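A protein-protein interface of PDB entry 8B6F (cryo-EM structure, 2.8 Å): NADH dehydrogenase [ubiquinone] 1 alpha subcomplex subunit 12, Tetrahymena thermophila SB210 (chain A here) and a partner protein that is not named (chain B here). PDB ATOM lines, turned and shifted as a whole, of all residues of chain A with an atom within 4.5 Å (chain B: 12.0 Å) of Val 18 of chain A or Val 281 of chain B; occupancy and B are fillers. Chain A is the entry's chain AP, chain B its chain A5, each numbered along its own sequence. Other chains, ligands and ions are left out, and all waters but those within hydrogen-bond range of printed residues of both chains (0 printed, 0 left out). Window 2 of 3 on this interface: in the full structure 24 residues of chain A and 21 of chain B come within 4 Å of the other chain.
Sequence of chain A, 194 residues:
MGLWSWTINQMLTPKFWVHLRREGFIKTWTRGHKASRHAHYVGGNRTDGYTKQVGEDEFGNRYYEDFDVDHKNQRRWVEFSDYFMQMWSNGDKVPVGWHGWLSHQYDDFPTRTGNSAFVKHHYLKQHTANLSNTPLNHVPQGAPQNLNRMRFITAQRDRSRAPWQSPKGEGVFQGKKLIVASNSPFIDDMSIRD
N of Val 280 of chain B lies within hydrogen-bond range of O of Tyr 50 of chain A (3.0 Å).
The chain-end carboxylate of Glu 282 of chain B lies within salt-bridge range of the guanidinium group of Arg 22 of chain A, 2.5 Å away.
Among the printed residues, merely in contact across the chains: Val 18 of chain A with Val 280 of chain B, Val 18 of chain A with Val 281 of chain B, Val 18 of chain A with Glu 282 of chain B, Asp 48 of chain A with Leu 279 of chain B, Asp 48 of chain A with Val 281 of chain B and Tyr 50 of chain A with Leu 279 of chain B.
No residue of chain B comes within 4 Å of Pro 14 of chain A.
No residue of chain B comes within 4 Å of Phe 16 of chain A.
No residue of chain B comes within 4 Å of Leu 20 of chain A.
No residue of chain B comes within 4 Å of Arg 21 of chain A.
Of chain B, only Leu 279 and Val 281 come within 4 Å of Asp 48 of chain A.
Tyr 50 of chain A touches just these residues of chain B: Leu 279 and Val 280.
Of the printed residues of chain A, Glu 282 of chain B touches Val 18 and Arg 22.
Printed residues of chain A within 4 Å of Val 280 of chain B: Val 18 (3.8 Å) and Tyr 50 (3.0 Å).
The nearest printed residue of chain A that does not touch Val 280 of chain B is Arg 22 of chain A (4.7 Å).
Of the 7 printed residues of chain B, 4 touch a printed residue of chain A.
Hydrophobic or aromatic side chains of chain B that line the printed part of chain A: Leu 279, Val 280 and Val 281.
Of the 11 printed residues of chain A, 4 touch a printed residue of chain B.
Among the printed residues, no Asp or Glu carboxylate lies within 4 Å of a Lys or Arg side-chain nitrogen of the other chain.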
ATOM      1  N   PRO A  14       7.154  14.234  23.328  1.00  0.00           N
ATOM      2  CA  PRO A  14       6.001  14.884  22.683  1.00  0.00           C
ATOM      3  C   PRO A  14       5.767  16.307  23.151  1.00  0.00           C
ATOM      4  O   PRO A  14       5.283  17.134  22.370  1.00  0.00           O
ATOM      5  CB  PRO A  14       4.828  13.967  23.057  1.00  0.00           C
ATOM      6  CG  PRO A  14       5.448  12.653  23.352  1.00  0.00           C
ATOM      7  CD  PRO A  14       6.784  12.954  23.954  1.00  0.00           C
ATOM      8  N   LYS A  15       6.093  16.620  24.406  1.00  0.00           N
ATOM      9  CA  LYS A  15       5.830  17.959  24.924  1.00  0.00           C
ATOM     10  C   LYS A  15       6.540  19.022  24.097  1.00  0.00           C
ATOM     11  O   LYS A  15       5.952  20.059  23.771  1.00  0.00           O
ATOM     12  CB  LYS A  15       6.257  18.050  26.390  1.00  0.00           C
ATOM     13  CG  LYS A  15       7.703  17.646  26.638  1.00  0.00           C
ATOM     14  CD  LYS A  15       8.085  17.768  28.102  1.00  0.00           C
ATOM     15  CE  LYS A  15       8.189  19.218  28.534  1.00  0.00           C
ATOM     16  NZ  LYS A  15       8.758  19.332  29.904  1.00  0.00           N
ATOM     17  N   PHE A  16       7.807  18.790  23.755  1.00  0.00           N
ATOM     18  CA  PHE A  16       8.550  19.781  22.986  1.00  0.00           C
ATOM     19  C   PHE A  16       7.905  20.026  21.630  1.00  0.00           C
ATOM     20  O   PHE A  16       7.789  21.174  21.187  1.00  0.00           O
ATOM     21  CB  PHE A  16       9.998  19.332  22.810  1.00  0.00           C
ATOM     22  CG  PHE A  16      10.760  20.138  21.802  1.00  0.00           C
ATOM     23  CD1 PHE A  16      11.215  21.407  22.112  1.00  0.00           C
ATOM     24  CD2 PHE A  16      11.026  19.625  20.545  1.00  0.00           C
ATOM     25  CE1 PHE A  16      11.917  22.152  21.187  1.00  0.00           C
ATOM     26  CE2 PHE A  16      11.727  20.365  19.614  1.00  0.00           C
ATOM     27  CZ  PHE A  16      12.173  21.629  19.937  1.00  0.00           C
ATOM     28  N   TRP A  17       7.478  18.959  20.955  1.00  0.00           N
ATOM     29  CA  TRP A  17       6.914  19.117  19.619  1.00  0.00           C
ATOM     30  C   TRP A  17       5.577  19.846  19.667  1.00  0.00           C
ATOM     31  O   TRP A  17       5.305  20.707  18.822  1.00  0.00           O
ATOM     32  CB  TRP A  17       6.774  17.750  18.952  1.00  0.00           C
ATOM     33  CG  TRP A  17       8.092  17.063  18.790  1.00  0.00           C
ATOM     34  CD1 TRP A  17       8.557  16.001  19.510  1.00  0.00           C
ATOM     35  CD2 TRP A  17       9.131  17.403  17.861  1.00  0.00           C
ATOM     36  NE1 TRP A  17       9.815  15.653  19.081  1.00  0.00           N
ATOM     37  CE2 TRP A  17      10.190  16.498  18.069  1.00  0.00           C
ATOM     38  CE3 TRP A  17       9.263  18.381  16.869  1.00  0.00           C
ATOM     39  CZ2 TRP A  17      11.368  16.542  17.324  1.00  0.00           C
ATOM     40  CZ3 TRP A  17      10.433  18.424  16.129  1.00  0.00           C
ATOM     41  CH2 TRP A  17      11.471  17.510  16.361  1.00  0.00           C
ATOM     42  N   VAL A  18       4.728  19.517  20.640  1.00  0.00           N
ATOM     43  CA  VAL A  18       3.457  20.222  20.774  1.00  0.00           C
ATOM     44  C   VAL A  18       3.700  21.691  21.086  1.00  0.00           C
ATOM     45  O   VAL A  18       3.047  22.579  20.525  1.00  0.00           O
ATOM     46  CB  VAL A  18       2.582  19.552  21.849  1.00  0.00           C
ATOM     47  CG1 VAL A  18       1.282  20.323  22.041  1.00  0.00           C
ATOM     48  CG2 VAL A  18       2.290  18.111  21.470  1.00  0.00           C
ATOM     49  N   HIS A  19       4.635  21.973  21.996  1.00  0.00           N
ATOM     50  CA  HIS A  19       4.930  23.357  22.347  1.00  0.00           C
ATOM     51  C   HIS A  19       5.470  24.126  21.148  1.00  0.00           C
ATOM     52  O   HIS A  19       5.087  25.278  20.915  1.00  0.00           O
ATOM     53  CB  HIS A  19       5.927  23.402  23.506  1.00  0.00           C
ATOM     54  CG  HIS A  19       5.878  24.675  24.289  1.00  0.00           C
ATOM     55  ND1 HIS A  19       6.413  25.857  23.823  1.00  0.00           N
ATOM     56  CD2 HIS A  19       5.354  24.954  25.505  1.00  0.00           C
ATOM     57  CE1 HIS A  19       6.220  26.808  24.719  1.00  0.00           C
ATOM     58  NE2 HIS A  19       5.581  26.286  25.749  1.00  0.00           N
ATOM     59  N   LEU A  20       6.356  23.500  20.372  1.00  0.00           N
ATOM     60  CA  LEU A  20       6.884  24.144  19.175  1.00  0.00           C
ATOM     61  C   LEU A  20       5.776  24.409  18.164  1.00  0.00           C
ATOM     62  O   LEU A  20       5.715  25.487  17.564  1.00  0.00           O
ATOM     63  CB  LEU A  20       7.979  23.273  18.557  1.00  0.00           C
ATOM     64  CG  LEU A  20       9.023  23.929  17.643  1.00  0.00           C
ATOM     65  CD1 LEU A  20      10.016  22.887  17.161  1.00  0.00           C
ATOM     66  CD2 LEU A  20       8.412  24.658  16.456  1.00  0.00           C
ATOM     67  N   ARG A  21       4.872  23.448  17.984  1.00  0.00           N
ATOM     68  CA  ARG A  21       3.792  23.623  17.022  1.00  0.00           C
ATOM     69  C   ARG A  21       2.885  24.784  17.407  1.00  0.00           C
ATOM     70  O   ARG A  21       2.480  25.574  16.546  1.00  0.00           O
ATOM     71  CB  ARG A  21       2.984  22.332  16.910  1.00  0.00           C
ATOM     72  CG  ARG A  21       1.963  22.327  15.786  1.00  0.00           C
ATOM     73  CD  ARG A  21       0.882  21.294  16.046  1.00  0.00           C
ATOM     74  NE  ARG A  21       1.446  19.996  16.398  1.00  0.00           N
ATOM     75  CZ  ARG A  21       0.738  18.965  16.837  1.00  0.00           C
ATOM     76  NH1 ARG A  21      -0.573  19.043  16.995  1.00  0.00           N
ATOM     77  NH2 ARG A  21       1.361  17.827  17.128  1.00  0.00           N
ATOM     78  N   ARG A  22       2.551  24.909  18.691  1.00  0.00           N
ATOM     79  CA  ARG A  22       1.576  25.905  19.123  1.00  0.00           C
ATOM     80  C   ARG A  22       2.223  27.258  19.410  1.00  0.00           C
ATOM     81  O   ARG A  22       1.889  28.258  18.766  1.00  0.00           O
ATOM     82  CB  ARG A  22       0.822  25.395  20.357  1.00  0.00           C
ATOM     83  CG  ARG A  22      -0.090  26.436  20.984  1.00  0.00           C
ATOM     84  CD  ARG A  22      -1.269  25.802  21.704  1.00  0.00           C
ATOM     85  NE  ARG A  22      -2.422  25.653  20.823  1.00  0.00           N
ATOM     86  CZ  ARG A  22      -2.723  24.554  20.143  1.00  0.00           C
ATOM     87  NH1 ARG A  22      -1.985  23.460  20.227  1.00  0.00           N
ATOM     88  NH2 ARG A  22      -3.796  24.553  19.357  1.00  0.00           N
ATOM     89  N   ASP A  48       4.452  13.760  28.316  1.00  0.00           N
ATOM     90  CA  ASP A  48       3.390  13.684  27.319  1.00  0.00           C
ATOM     91  C   ASP A  48       2.781  15.042  26.997  1.00  0.00           C
ATOM     92  O   ASP A  48       2.019  15.142  26.031  1.00  0.00           O
ATOM     93  CB  ASP A  48       2.294  12.726  27.793  1.00  0.00           C
ATOM     94  CG  ASP A  48       1.793  13.057  29.182  1.00  0.00           C
ATOM     95  OD1 ASP A  48       2.582  13.597  29.983  1.00  0.00           O
ATOM     96  OD2 ASP A  48       0.613  12.771  29.476  1.00  0.00           O
ATOM     97  N   TYR A  50       2.959  19.676  28.143  1.00  0.00           N
ATOM     98  CA  TYR A  50       3.515  20.769  28.925  1.00  0.00           C
ATOM     99  C   TYR A  50       2.437  21.398  29.798  1.00  0.00           C
ATOM    100  O   TYR A  50       1.262  21.450  29.425  1.00  0.00           O
ATOM    101  CB  TYR A  50       4.153  21.833  28.024  1.00  0.00           C
ATOM    102  CG  TYR A  50       3.197  22.551  27.104  1.00  0.00           C
ATOM    103  CD1 TYR A  50       2.905  22.048  25.845  1.00  0.00           C
ATOM    104  CD2 TYR A  50       2.613  23.750  27.483  1.00  0.00           C
ATOM    105  CE1 TYR A  50       2.043  22.711  24.995  1.00  0.00           C
ATOM    106  CE2 TYR A  50       1.749  24.421  26.642  1.00  0.00           C
ATOM    107  CZ  TYR A  50       1.469  23.898  25.400  1.00  0.00           C
ATOM    108  OH  TYR A  50       0.609  24.563  24.560  1.00  0.00           O
ATOM    109  N   ARG B 276      -4.480  16.618  39.925  1.00  0.00           N
ATOM    110  CA  ARG B 276      -3.707  16.314  38.730  1.00  0.00           C
ATOM    111  C   ARG B 276      -3.242  17.614  38.094  1.00  0.00           C
ATOM    112  O   ARG B 276      -3.821  18.681  38.314  1.00  0.00           O
ATOM    113  CB  ARG B 276      -4.523  15.487  37.731  1.00  0.00           C
ATOM    114  CG  ARG B 276      -5.843  16.124  37.334  1.00  0.00           C
ATOM    115  CD  ARG B 276      -6.569  15.292  36.292  1.00  0.00           C
ATOM    116  NE  ARG B 276      -5.817  15.206  35.045  1.00  0.00           N
ATOM    117  CZ  ARG B 276      -5.836  16.124  34.089  1.00  0.00           C
ATOM    118  NH1 ARG B 276      -6.559  17.226  34.201  1.00  0.00           N
ATOM    119  NH2 ARG B 276      -5.107  15.935  32.993  1.00  0.00           N
ATOM    120  N   THR B 277      -2.181  17.510  37.299  1.00  0.00           N
ATOM    121  CA  THR B 277      -1.620  18.668  36.619  1.00  0.00           C
ATOM    122  C   THR B 277      -2.363  18.924  35.315  1.00  0.00           C
ATOM    123  O   THR B 277      -2.620  17.995  34.544  1.00  0.00           O
ATOM    124  CB  THR B 277      -0.135  18.451  36.332  1.00  0.00           C
ATOM    125  OG1 THR B 277       0.565  18.192  37.554  1.00  0.00           O
ATOM    126  CG2 THR B 277       0.468  19.677  35.660  1.00  0.00           C
ATOM    127  N   ASN B 278      -2.714  20.184  35.074  1.00  0.00           N
ATOM    128  CA  ASN B 278      -3.290  20.564  33.793  1.00  0.00           C
ATOM    129  C   ASN B 278      -2.219  20.512  32.714  1.00  0.00           C
ATOM    130  O   ASN B 278      -1.124  21.054  32.887  1.00  0.00           O
ATOM    131  CB  ASN B 278      -3.893  21.964  33.875  1.00  0.00           C
ATOM    132  CG  ASN B 278      -5.002  22.059  34.898  1.00  0.00           C
ATOM    133  OD1 ASN B 278      -4.878  22.760  35.902  1.00  0.00           O
ATOM    134  ND2 ASN B 278      -6.098  21.352  34.647  1.00  0.00           N
ATOM    135  N   LEU B 279      -2.533  19.859  31.600  1.00  0.00           N
ATOM    136  CA  LEU B 279      -1.586  19.680  30.511  1.00  0.00           C
ATOM    137  C   LEU B 279      -2.217  20.076  29.188  1.00  0.00           C
ATOM    138  O   LEU B 279      -3.428  19.953  28.994  1.00  0.00           O
ATOM    139  CB  LEU B 279      -1.104  18.239  30.406  1.00  0.00           C
ATOM    140  CG  LEU B 279      -0.296  17.682  31.570  1.00  0.00           C
ATOM    141  CD1 LEU B 279       0.084  16.273  31.210  1.00  0.00           C
ATOM    142  CD2 LEU B 279       0.935  18.521  31.878  1.00  0.00           C
ATOM    143  N   VAL B 280      -1.373  20.559  28.280  1.00  0.00           N
ATOM    144  CA  VAL B 280      -1.785  20.836  26.911  1.00  0.00           C
ATOM    145  C   VAL B 280      -1.202  19.748  26.022  1.00  0.00           C
ATOM    146  O   VAL B 280      -0.057  19.850  25.569  1.00  0.00           O
ATOM    147  CB  VAL B 280      -1.327  22.234  26.462  1.00  0.00           C
ATOM    148  CG1 VAL B 280      -1.731  22.491  25.017  1.00  0.00           C
ATOM    149  CG2 VAL B 280      -1.893  23.301  27.385  1.00  0.00           C
ATOM    150  N   VAL B 281      -1.984  18.695  25.770  1.00  0.00           N
ATOM    151  CA  VAL B 281      -1.487  17.552  25.008  1.00  0.00           C
ATOM    152  C   VAL B 281      -1.598  17.757  23.507  1.00  0.00           C
ATOM    153  O   VAL B 281      -0.983  17.003  22.742  1.00  0.00           O
ATOM    154  CB  VAL B 281      -2.242  16.270  25.410  1.00  0.00           C
ATOM    155  CG1 VAL B 281      -1.572  15.034  24.819  1.00  0.00           C
ATOM    156  CG2 VAL B 281      -2.333  16.150  26.925  1.00  0.00           C
ATOM    157  N   GLU B 282      -2.346  18.761  23.061  1.00  0.00           N
ATOM    158  CA  GLU B 282      -2.484  19.037  21.638  1.00  0.00           C
ATOM    159  C   GLU B 282      -2.456  20.538  21.373  1.00  0.00           C
ATOM    160  O   GLU B 282      -2.815  21.342  22.233  1.00  0.00           O
ATOM    161  CB  GLU B 282      -3.782  18.432  21.098  1.00  0.00           C
ATOM    162  CG  GLU B 282      -3.888  16.927  21.300  1.00  0.00           C
ATOM    163  CD  GLU B 282      -5.127  16.339  20.654  1.00  0.00           C
ATOM    164  OE1 GLU B 282      -5.791  17.056  19.876  1.00  0.00           O
ATOM    165  OE2 GLU B 282      -5.439  15.160  20.925  1.00  0.00           O
ATOM    166  OXT GLU B 282      -2.074  20.983  20.291  1.00  0.00           O
